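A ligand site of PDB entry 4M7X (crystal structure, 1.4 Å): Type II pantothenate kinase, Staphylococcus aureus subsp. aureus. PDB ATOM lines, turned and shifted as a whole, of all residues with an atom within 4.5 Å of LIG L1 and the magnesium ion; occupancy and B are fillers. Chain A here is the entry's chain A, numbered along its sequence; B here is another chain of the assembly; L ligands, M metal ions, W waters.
Water W8 bridges OD2 of Asp 6 and NZ of Lys 13.
Water W1 lies within hydrogen-bond range of an oxygen (O7) of LIG L1 and the guanidinium group (NH1) of Arg 113.
Water W3 bridges O2 of LIG L1 and O of Gly 100.
Water W10 bridges the side-chain carboxylate of Glu 70 and an oxygen (O1) of LIG L1.
Water W6 lies within hydrogen-bond range of OH of Tyr 240 of chain B (2.7 Å), OG1 of Thr 206 of chain B (2.7 Å) and O of Gly 116 (3.0 Å).
A nitrogen (N2) of LIG L1 lies within hydrogen-bond range of the backbone carbonyl oxygen of Thr 172 of chain B (2.9 Å).
The guanidinium group of Arg 113 sits at hydrogen-bond distance from an oxygen (O6) of LIG L1.
The backbone NH (N) of Gly 100 lies within hydrogen-bond range of an oxygen (O2) of LIG L1, 3.2 Å away.
An oxygen (O1) of LIG L1 is in hydrogen-bond range of the backbone NH (N) of Gly 9, 3.2 Å away.
An oxygen (O2) of LIG L1 sits at hydrogen-bond distance from the backbone NH (N) of Thr 99, at 3.3 Å.
The backbone carbonyl oxygen (O) of Ala 173 of chain B lies within hydrogen-bond range of a nitrogen (N1) of LIG L1.
O1 of LG2 L2 sits at hydrogen-bond distance from N of Gly 9.
O1 of LG2 L2 sits at hydrogen-bond distance from N of Thr 99, at 3.2 Å.
O1 of LG2 L2 is in hydrogen-bond range of OG1 of Thr 99 (2.5 Å).
The side-chain amino group (NZ) of Lys 13 lies within salt-bridge range of an oxygen (O4) of LG2 L2 (2.8 Å).
The magnesium ion is bound by O3 of LIG L1 (1.9 Å), water W8 (2.0 Å), O2 of LG2 L2 (2.1 Å), water W7 (2.1 Å), water W9 (2.1 Å) and water W2 (2.2 Å).
OE2 of Glu 202 of chain B lies within hydrogen-bond range of OG1 of Thr 172 of chain B, 2.8 Å away.
The side-chain hydroxyl (OG) of Ser 102 is in hydrogen-bond range of the guanidinium group (NE) of Arg 113, 2.8 Å away.
The backbone NH of Ile 117 is in hydrogen-bond range of the backbone carbonyl oxygen of Thr 101.
The backbone carbonyl oxygen (O) of Glu 202 of chain B is in hydrogen-bond range of the side-chain hydroxyl (OG1) of Thr 206 of chain B (2.7 Å).
The backbone carbonyl oxygen (O) of Leu 171 of chain B is in hydrogen-bond range of the backbone NH (N) of Val 156 of chain B.
Glu 70 touches the magnesium ion (OE1 to MG, 3.9 Å).
Of the 24 residues printed, 1 comes within 4 Å of the magnesium ion.
OE1 of Glu 70 lies close to O4 of LIG L1.
Residues that only touch LIG L1: Phe 71 (3.8 Å), Gly 98 (3.9 Å), Thr 101 (3.5 Å), Ser 102 (3.4 Å), Gly 116 (3.4 Å), Ile 117 (3.4 Å), Val 156 of chain B (3.8 Å), Ile 167 of chain B (3.9 Å), Leu 171 of chain B (3.98 Å), Glu 202 of chain B (3.5 Å) and Tyr 240 of chain B (3.3 Å).
Hydrophobic or aromatic side chains within 4 Å of LIG L1: Phe 71, Val 156 of chain B, Ile 167 of chain B, Leu 171 of chain B and Tyr 240 of chain B.
18 residues have an atom within 4 Å of LIG L1: Gly 9, Glu 70, Phe 71, Gly 98, Thr 99, Gly 100, Thr 101, Ser 102, Arg 113, Gly 116, Ile 117, Val 156 of chain B, Ile 167 of chain B, Leu 171 of chain B, Thr 172 of chain B, Ala 173 of chain B, Glu 202 of chain B and Tyr 240 of chain B.
The nearest printed residue that does not touch LIG L1 is Ile 159 of chain B (4.03 Å).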
ATOM      1  N   ASP A   6      20.550  -6.642  29.189  1.00  0.00           N
ATOM      2  CA  ASP A   6      19.482  -6.865  28.229  1.00  0.00           C
ATOM      3  C   ASP A   6      18.215  -6.719  29.084  1.00  0.00           C
ATOM      4  O   ASP A   6      17.843  -7.605  29.841  1.00  0.00           O
ATOM      5  CB  ASP A   6      19.606  -8.258  27.606  1.00  0.00           C
ATOM      6  CG  ASP A   6      18.489  -8.588  26.687  1.00  0.00           C
ATOM      7  OD1 ASP A   6      17.564  -7.786  26.553  1.00  0.00           O
ATOM      8  OD2 ASP A   6      18.543  -9.646  26.063  1.00  0.00           O
ATOM      9  N   GLY A   8      14.695  -6.725  29.088  1.00  0.00           N
ATOM     10  CA  GLY A   8      13.593  -7.214  28.252  1.00  0.00           C
ATOM     11  C   GLY A   8      12.220  -6.917  28.809  1.00  0.00           C
ATOM     12  O   GLY A   8      12.058  -6.193  29.784  1.00  0.00           O
ATOM     13  N   GLY A   9      11.212  -7.523  28.203  1.00  0.00           N
ATOM     14  CA  GLY A   9       9.848  -7.299  28.623  1.00  0.00           C
ATOM     15  C   GLY A   9       9.478  -7.855  29.975  1.00  0.00           C
ATOM     16  O   GLY A   9       8.607  -7.320  30.632  1.00  0.00           O
ATOM     17  N   LYS A  13      18.495  -9.150  32.205  1.00  0.00           N
ATOM     18  CA  LYS A  13      19.616 -10.058  32.242  1.00  0.00           C
ATOM     19  C   LYS A  13      20.860  -9.226  32.307  1.00  0.00           C
ATOM     20  O   LYS A  13      21.075  -8.348  31.436  1.00  0.00           O
ATOM     21  CB  LYS A  13      19.678 -10.935  30.963  1.00  0.00           C
ATOM     22  CG  LYS A  13      18.748 -12.129  30.963  1.00  0.00           C
ATOM     23  CD  LYS A  13      17.290 -11.793  30.819  1.00  0.00           C
ATOM     24  CE  LYS A  13      17.006 -11.071  29.503  1.00  0.00           C
ATOM     25  NZ  LYS A  13      15.555 -10.898  29.258  1.00  0.00           N
ATOM     26  N   GLU A  70      18.481  -5.213  19.876  1.00  0.00           N
ATOM     27  CA  GLU A  70      18.511  -6.507  20.517  1.00  0.00           C
ATOM     28  C   GLU A  70      18.759  -7.612  19.553  1.00  0.00           C
ATOM     29  O   GLU A  70      19.321  -8.612  19.943  1.00  0.00           O
ATOM     30  CB  GLU A  70      17.253  -6.809  21.394  1.00  0.00           C
ATOM     31  CG  GLU A  70      15.935  -7.012  20.664  1.00  0.00           C
ATOM     32  CD  GLU A  70      14.816  -7.444  21.610  1.00  0.00           C
ATOM     33  OE1 GLU A  70      14.690  -8.659  21.909  1.00  0.00           O
ATOM     34  OE2 GLU A  70      14.058  -6.570  22.062  1.00  0.00           O
ATOM     35  N   PHE A  71      18.274  -7.490  18.303  1.00  0.00           N
ATOM     36  CA  PHE A  71      18.405  -8.621  17.359  1.00  0.00           C
ATOM     37  C   PHE A  71      19.860  -8.879  17.023  1.00  0.00           C
ATOM     38  O   PHE A  71      20.303 -10.039  17.024  1.00  0.00           O
ATOM     39  CB  PHE A  71      17.596  -8.424  16.088  1.00  0.00           C
ATOM     40  CG  PHE A  71      16.123  -8.163  16.329  1.00  0.00           C
ATOM     41  CD1 PHE A  71      15.427  -8.794  17.361  1.00  0.00           C
ATOM     42  CD2 PHE A  71      15.415  -7.306  15.476  1.00  0.00           C
ATOM     43  CE1 PHE A  71      14.071  -8.555  17.559  1.00  0.00           C
ATOM     44  CE2 PHE A  71      14.056  -7.094  15.660  1.00  0.00           C
ATOM     45  CZ  PHE A  71      13.403  -7.686  16.696  1.00  0.00           C
ATOM     46  N   GLY A  98      11.255 -15.376  24.394  1.00  0.00           N
ATOM     47  CA  GLY A  98      11.236 -14.466  25.521  1.00  0.00           C
ATOM     48  C   GLY A  98       9.839 -14.236  25.968  1.00  0.00           C
ATOM     49  O   GLY A  98       9.023 -15.171  25.968  1.00  0.00           O
ATOM     50  N   THR A  99       9.499 -12.982  26.295  1.00  0.00           N
ATOM     51  CA  THR A  99       8.138 -12.652  26.609  1.00  0.00           C
ATOM     52  C   THR A  99       7.243 -13.044  25.418  1.00  0.00           C
ATOM     53  O   THR A  99       6.184 -13.618  25.603  1.00  0.00           O
ATOM     54  CB  THR A  99       7.985 -11.174  26.950  1.00  0.00           C
ATOM     55  OG1 THR A  99       8.864 -10.856  28.084  1.00  0.00           O
ATOM     56  CG2 THR A  99       6.617 -10.882  27.343  1.00  0.00           C
ATOM     57  N   GLY A 100       7.715 -12.717  24.230  1.00  0.00           N
ATOM     58  CA  GLY A 100       7.214 -13.254  22.987  1.00  0.00           C
ATOM     59  C   GLY A 100       8.343 -13.883  22.189  1.00  0.00           C
ATOM     60  O   GLY A 100       9.484 -13.893  22.661  1.00  0.00           O
ATOM     61  N   THR A 101       8.063 -14.364  20.983  1.00  0.00           N
ATOM     62  CA  THR A 101       9.048 -15.148  20.248  1.00  0.00           C
ATOM     63  C   THR A 101       9.467 -14.458  18.975  1.00  0.00           C
ATOM     64  O   THR A 101       8.620 -14.095  18.130  1.00  0.00           O
ATOM     65  CB  THR A 101       8.527 -16.539  19.956  1.00  0.00           C
ATOM     66  OG1 THR A 101       8.283 -17.193  21.212  1.00  0.00           O
ATOM     67  CG2 THR A 101       9.471 -17.314  19.099  1.00  0.00           C
ATOM     68  N   SER A 102      10.768 -14.322  18.785  1.00  0.00           N
ATOM     69  CA  SER A 102      11.361 -13.727  17.578  1.00  0.00           C
ATOM     70  C   SER A 102      12.217 -14.775  16.893  1.00  0.00           C
ATOM     71  O   SER A 102      12.987 -15.457  17.570  1.00  0.00           O
ATOM     72  CB  SER A 102      12.183 -12.530  18.021  1.00  0.00           C
ATOM     73  OG  SER A 102      12.578 -11.779  16.898  1.00  0.00           O
ATOM     74  N   ARG A 113      15.771 -11.113  10.772  1.00  0.00           N
ATOM     75  CA  ARG A 113      14.556 -11.568  11.403  1.00  0.00           C
ATOM     76  C   ARG A 113      13.649 -12.079  10.325  1.00  0.00           C
ATOM     77  O   ARG A 113      13.422 -11.389   9.286  1.00  0.00           O
ATOM     78  CB  ARG A 113      13.864 -10.463  12.171  1.00  0.00           C
ATOM     79  CG  ARG A 113      12.727 -10.920  13.045  1.00  0.00           C
ATOM     80  CD  ARG A 113      12.250  -9.775  13.929  1.00  0.00           C
ATOM     81  NE  ARG A 113      11.294 -10.172  14.957  1.00  0.00           N
ATOM     82  CZ  ARG A 113       9.986 -10.285  14.759  1.00  0.00           C
ATOM     83  NH1 ARG A 113       9.444 -10.020  13.602  1.00  0.00           N
ATOM     84  NH2 ARG A 113       9.228 -10.629  15.760  1.00  0.00           N
ATOM     85  N   GLY A 116       7.983 -13.922  13.733  1.00  0.00           N
ATOM     86  CA  GLY A 116       7.784 -13.838  15.132  1.00  0.00           C
ATOM     87  C   GLY A 116       6.358 -14.151  15.456  1.00  0.00           C
ATOM     88  O   GLY A 116       5.480 -14.192  14.560  1.00  0.00           O
ATOM     89  N   ILE A 117       6.096 -14.369  16.733  1.00  0.00           N
ATOM     90  CA  ILE A 117       4.743 -14.724  17.177  1.00  0.00           C
ATOM     91  C   ILE A 117       4.600 -14.407  18.646  1.00  0.00           C
ATOM     92  O   ILE A 117       5.592 -14.407  19.379  1.00  0.00           O
ATOM     93  CB  ILE A 117       4.459 -16.207  16.873  1.00  0.00           C
ATOM     94  CG1 ILE A 117       2.980 -16.544  16.997  1.00  0.00           C
ATOM     95  CG2 ILE A 117       5.365 -17.127  17.630  1.00  0.00           C
ATOM     96  CD1 ILE A 117       2.083 -15.786  16.056  1.00  0.00           C
ATOM     97  N   GLY A 118       3.383 -14.097  19.114  1.00  0.00           N
ATOM     98  CA  GLY A 118       3.186 -13.722  20.499  1.00  0.00           C
ATOM     99  C   GLY A 118       3.016 -14.891  21.450  1.00  0.00           C
ATOM    100  O   GLY A 118       2.692 -14.733  22.623  1.00  0.00           O
ATOM    101  N   VAL B 156       4.194  -4.659  21.328  1.00  0.00           N
ATOM    102  CA  VAL B 156       5.591  -4.279  21.235  1.00  0.00           C
ATOM    103  C   VAL B 156       5.878  -2.908  21.924  1.00  0.00           C
ATOM    104  O   VAL B 156       6.871  -2.751  22.631  1.00  0.00           O
ATOM    105  CB  VAL B 156       6.024  -4.252  19.725  1.00  0.00           C
ATOM    106  CG1 VAL B 156       7.420  -3.673  19.558  1.00  0.00           C
ATOM    107  CG2 VAL B 156       5.977  -5.660  19.157  1.00  0.00           C
ATOM    108  N   ILE B 159       6.634  -2.842  25.608  1.00  0.00           N
ATOM    109  CA  ILE B 159       7.946  -3.253  26.016  1.00  0.00           C
ATOM    110  C   ILE B 159       8.934  -2.146  25.756  1.00  0.00           C
ATOM    111  O   ILE B 159       9.726  -1.794  26.617  1.00  0.00           O
ATOM    112  CB  ILE B 159       8.384  -4.557  25.298  1.00  0.00           C
ATOM    113  CG1 ILE B 159       7.387  -5.671  25.637  1.00  0.00           C
ATOM    114  CG2 ILE B 159       9.810  -4.942  25.649  1.00  0.00           C
ATOM    115  CD1 ILE B 159       7.693  -6.973  24.940  1.00  0.00           C
ATOM    116  N   ILE B 167      10.535  -3.332  15.390  1.00  0.00           N
ATOM    117  CA  ILE B 167       9.419  -3.816  14.593  1.00  0.00           C
ATOM    118  C   ILE B 167       8.203  -3.022  15.033  1.00  0.00           C
ATOM    119  O   ILE B 167       8.246  -2.418  16.108  1.00  0.00           O
ATOM    120  CB  ILE B 167       9.184  -5.327  14.775  1.00  0.00           C
ATOM    121  CG1 ILE B 167       8.865  -5.651  16.243  1.00  0.00           C
ATOM    122  CG2 ILE B 167      10.418  -6.118  14.323  1.00  0.00           C
ATOM    123  CD1 ILE B 167       8.591  -7.107  16.483  1.00  0.00           C
ATOM    124  N   LEU B 171       2.199  -4.271  16.948  1.00  0.00           N
ATOM    125  CA  LEU B 171       2.131  -5.712  16.857  1.00  0.00           C
ATOM    126  C   LEU B 171       1.973  -6.315  18.241  1.00  0.00           C
ATOM    127  O   LEU B 171       2.559  -5.830  19.193  1.00  0.00           O
ATOM    128  CB  LEU B 171       3.435  -6.238  16.269  1.00  0.00           C
ATOM    129  CG  LEU B 171       3.736  -5.937  14.826  1.00  0.00           C
ATOM    130  CD1 LEU B 171       5.104  -6.486  14.495  1.00  0.00           C
ATOM    131  CD2 LEU B 171       2.676  -6.530  13.947  1.00  0.00           C
ATOM    132  N   THR B 172       1.215  -7.425  18.329  1.00  0.00           N
ATOM    133  CA  THR B 172       1.200  -8.252  19.569  1.00  0.00           C
ATOM    134  C   THR B 172       2.593  -8.763  19.852  1.00  0.00           C
ATOM    135  O   THR B 172       3.166  -9.484  19.002  1.00  0.00           O
ATOM    136  CB  THR B 172       0.204  -9.399  19.454  1.00  0.00           C
ATOM    137  OG1 THR B 172      -1.069  -8.871  18.975  1.00  0.00           O
ATOM    138  CG2 THR B 172      -0.011 -10.105  20.766  1.00  0.00           C
ATOM    139  N   ALA B 173       3.131  -8.432  21.001  1.00  0.00           N
ATOM    140  CA  ALA B 173       4.405  -9.009  21.458  1.00  0.00           C
ATOM    141  C   ALA B 173       4.167 -10.299  22.150  1.00  0.00           C
ATOM    142  O   ALA B 173       4.934 -11.232  21.931  1.00  0.00           O
ATOM    143  CB  ALA B 173       5.135  -8.038  22.404  1.00  0.00           C
ATOM    144  N   GLU B 202      -4.004 -14.914  15.031  1.00  0.00           N
ATOM    145  CA  GLU B 202      -2.634 -14.457  14.799  1.00  0.00           C
ATOM    146  C   GLU B 202      -1.708 -15.596  14.399  1.00  0.00           C
ATOM    147  O   GLU B 202      -0.863 -15.413  13.552  1.00  0.00           O
ATOM    148  CB  GLU B 202      -2.090 -13.680  15.985  1.00  0.00           C
ATOM    149  CG  GLU B 202      -2.860 -12.389  16.246  1.00  0.00           C
ATOM    150  CD  GLU B 202      -2.341 -11.615  17.451  1.00  0.00           C
ATOM    151  OE1 GLU B 202      -1.416 -12.063  18.144  1.00  0.00           O
ATOM    152  OE2 GLU B 202      -2.884 -10.505  17.707  1.00  0.00           O
ATOM    153  N   THR B 206       0.004 -15.794  10.801  1.00  0.00           N
ATOM    154  CA  THR B 206       1.445 -15.780  10.751  1.00  0.00           C
ATOM    155  C   THR B 206       1.974 -16.970   9.962  1.00  0.00           C
ATOM    156  O   THR B 206       2.854 -16.815   9.125  1.00  0.00           O
ATOM    157  CB  THR B 206       2.022 -15.803  12.181  1.00  0.00           C
ATOM    158  OG1 THR B 206       1.624 -14.589  12.830  1.00  0.00           O
ATOM    159  CG2 THR B 206       3.540 -15.886  12.111  1.00  0.00           C
ATOM    160  N   TYR B 240      -4.228  -8.656   9.462  1.00  0.00           N
ATOM    161  CA  TYR B 240      -2.790  -9.003   9.545  1.00  0.00           C
ATOM    162  C   TYR B 240      -2.269  -9.535   8.206  1.00  0.00           C
ATOM    163  O   TYR B 240      -1.123  -9.270   7.830  1.00  0.00           O
ATOM    164  CB  TYR B 240      -2.481  -9.963  10.652  1.00  0.00           C
ATOM    165  CG  TYR B 240      -0.999 -10.098  10.918  1.00  0.00           C
ATOM    166  CD1 TYR B 240      -0.189  -8.943  11.115  1.00  0.00           C
ATOM    167  CD2 TYR B 240      -0.399 -11.340  11.023  1.00  0.00           C
ATOM    168  CE1 TYR B 240       1.169  -9.062  11.359  1.00  0.00           C
ATOM    169  CE2 TYR B 240       0.983 -11.460  11.271  1.00  0.00           C
ATOM    170  CZ  TYR B 240       1.742 -10.307  11.446  1.00  0.00           C
ATOM    171  OH  TYR B 240       3.088 -10.407  11.694  1.00  0.00           O
HETATM  172  O1  LIG L   1      11.294  -8.896  25.306  1.00  0.00           O
HETATM  173  P1  LIG L   1      11.529  -9.815  24.094  1.00  0.00           P
HETATM  174  O2  LIG L   1      10.463 -11.077  23.838  1.00  0.00           O
HETATM  175  O3  LIG L   1      12.941 -10.338  24.257  1.00  0.00           O
HETATM  176  O4  LIG L   1      11.551  -8.937  22.702  1.00  0.00           O
HETATM  177  C1  LIG L   1      10.531  -8.110  22.314  1.00  0.00           C
HETATM  178  C2  LIG L   1       9.986  -8.565  20.934  1.00  0.00           C
HETATM  179  C3  LIG L   1      11.043  -8.332  19.843  1.00  0.00           C
HETATM  180  C4  LIG L   1       8.744  -7.721  20.676  1.00  0.00           C
HETATM  181  C5  LIG L   1       9.547 -10.081  20.995  1.00  0.00           C
HETATM  182  O5  LIG L   1       8.657 -10.331  22.124  1.00  0.00           O
HETATM  183  C6  LIG L   1       8.810 -10.497  19.740  1.00  0.00           C
HETATM  184  O6  LIG L   1       9.410 -10.591  18.651  1.00  0.00           O
HETATM  185  N1  LIG L   1       7.508 -10.757  19.870  1.00  0.00           N
HETATM  186  C7  LIG L   1       6.686 -11.209  18.775  1.00  0.00           C
HETATM  187  C8  LIG L   1       6.317  -9.969  17.877  1.00  0.00           C
HETATM  188  C9  LIG L   1       5.649 -10.452  16.608  1.00  0.00           C
HETATM  189  O7  LIG L   1       6.303 -10.779  15.641  1.00  0.00           O
HETATM  190  N2  LIG L   1       4.333 -10.560  16.621  1.00  0.00           N
HETATM  191  C10 LIG L   1       3.625 -11.097  15.457  1.00  0.00           C
HETATM  192  C11 LIG L   1       2.167 -11.303  15.724  1.00  0.00           C
HETATM  193  C12 LIG L   1       1.565  -9.961  15.725  1.00  0.00           C
HETATM  194  C13 LIG L   1       0.644  -9.904  14.536  1.00  0.00           C
HETATM  195  C14 LIG L   1      -0.622  -9.467  15.198  1.00  0.00           C
HETATM  196  C15 LIG L   1      -1.388  -8.630  14.211  1.00  0.00           C
HETATM  197  C16 LIG L   1      -2.048  -7.537  15.060  1.00  0.00           C
HETATM  198  P1  LG2 L   2      12.403 -10.871  27.829  1.00  0.00           P
HETATM  199  O1  LG2 L   2      11.140 -10.409  27.106  1.00  0.00           O
HETATM  200  O2  LG2 L   2      13.708 -10.553  27.127  1.00  0.00           O
HETATM  201  O3  LG2 L   2      12.384 -10.407  29.270  1.00  0.00           O
HETATM  202  P2  LG2 L   2      13.216 -13.672  28.422  1.00  0.00           P
HETATM  203  O4  LG2 L   2      13.974 -13.161  29.631  1.00  0.00           O
HETATM  204  O5  LG2 L   2      14.057 -14.317  27.401  1.00  0.00           O
HETATM  205  O6  LG2 L   2      12.351 -12.487  27.893  1.00  0.00           O
HETATM  206  O7  LG2 L   2      12.035 -14.639  28.829  1.00  0.00           O
HETATM  207  C1  LG2 L   2      10.977 -14.198  29.687  1.00  0.00           C
HETATM  208  C2  LG2 L   2      10.181 -15.427  30.110  1.00  0.00           C
HETATM  209  O8  LG2 L   2      11.009 -16.337  30.839  1.00  0.00           O
HETATM  210  C3  LG2 L   2       8.998 -15.161  31.019  1.00  0.00           C
HETATM  211  O9  LG2 L   2       7.874 -14.684  30.290  1.00  0.00           O
HETATM  212  C4  LG2 L   2       8.818 -16.512  31.690  1.00  0.00           C
HETATM  213  O10 LG2 L   2       8.042 -17.417  30.903  1.00  0.00           O
HETATM  214  C5  LG2 L   2      10.253 -17.026  31.809  1.00  0.00           C
HETATM  215  N1  LG2 L   2      10.908 -16.821  33.119  1.00  0.00           N
HETATM  216  C6  LG2 L   2      12.015 -17.542  33.408  1.00  0.00           C
HETATM  217  N2  LG2 L   2      12.403 -17.269  34.675  1.00  0.00           N
HETATM  218  C7  LG2 L   2      11.570 -16.375  35.186  1.00  0.00           C
HETATM  219  C8  LG2 L   2      11.392 -15.671  36.461  1.00  0.00           C
HETATM  220  N3  LG2 L   2      12.283 -15.879  37.475  1.00  0.00           N
HETATM  221  N4  LG2 L   2      10.363 -14.839  36.604  1.00  0.00           N
HETATM  222  C9  LG2 L   2       9.460 -14.618  35.618  1.00  0.00           C
HETATM  223  N5  LG2 L   2       9.539 -15.211  34.408  1.00  0.00           N
HETATM  224  C10 LG2 L   2      10.546 -16.093  34.178  1.00  0.00           C
HETATM  225 MG    MG M   1      14.582 -10.628  25.261  1.00  0.00          MG
HETATM  226  O   HOH W   1       6.553 -10.463  12.945  1.00  0.00           O
HETATM  227  O   HOH W   2      14.206 -12.736  25.034  1.00  0.00           O
HETATM  228  O   HOH W   3      12.353 -12.643  22.232  1.00  0.00           O
HETATM  229  O   HOH W   4      -4.748  -9.123  16.236  1.00  0.00           O
HETATM  230  O   HOH W   5      -4.432  -6.543  17.280  1.00  0.00           O
HETATM  231  O   HOH W   6       3.718 -12.856  12.570  1.00  0.00           O
HETATM  232  O   HOH W   7      15.496 -10.670  23.386  1.00  0.00           O
HETATM  233  O   HOH W   8      16.314 -11.122  26.148  1.00  0.00           O
HETATM  234  O   HOH W   9      15.136  -8.567  25.390  1.00  0.00           O
HETATM  235  O   HOH W  10      13.191  -6.565  24.614  1.00  0.00           O
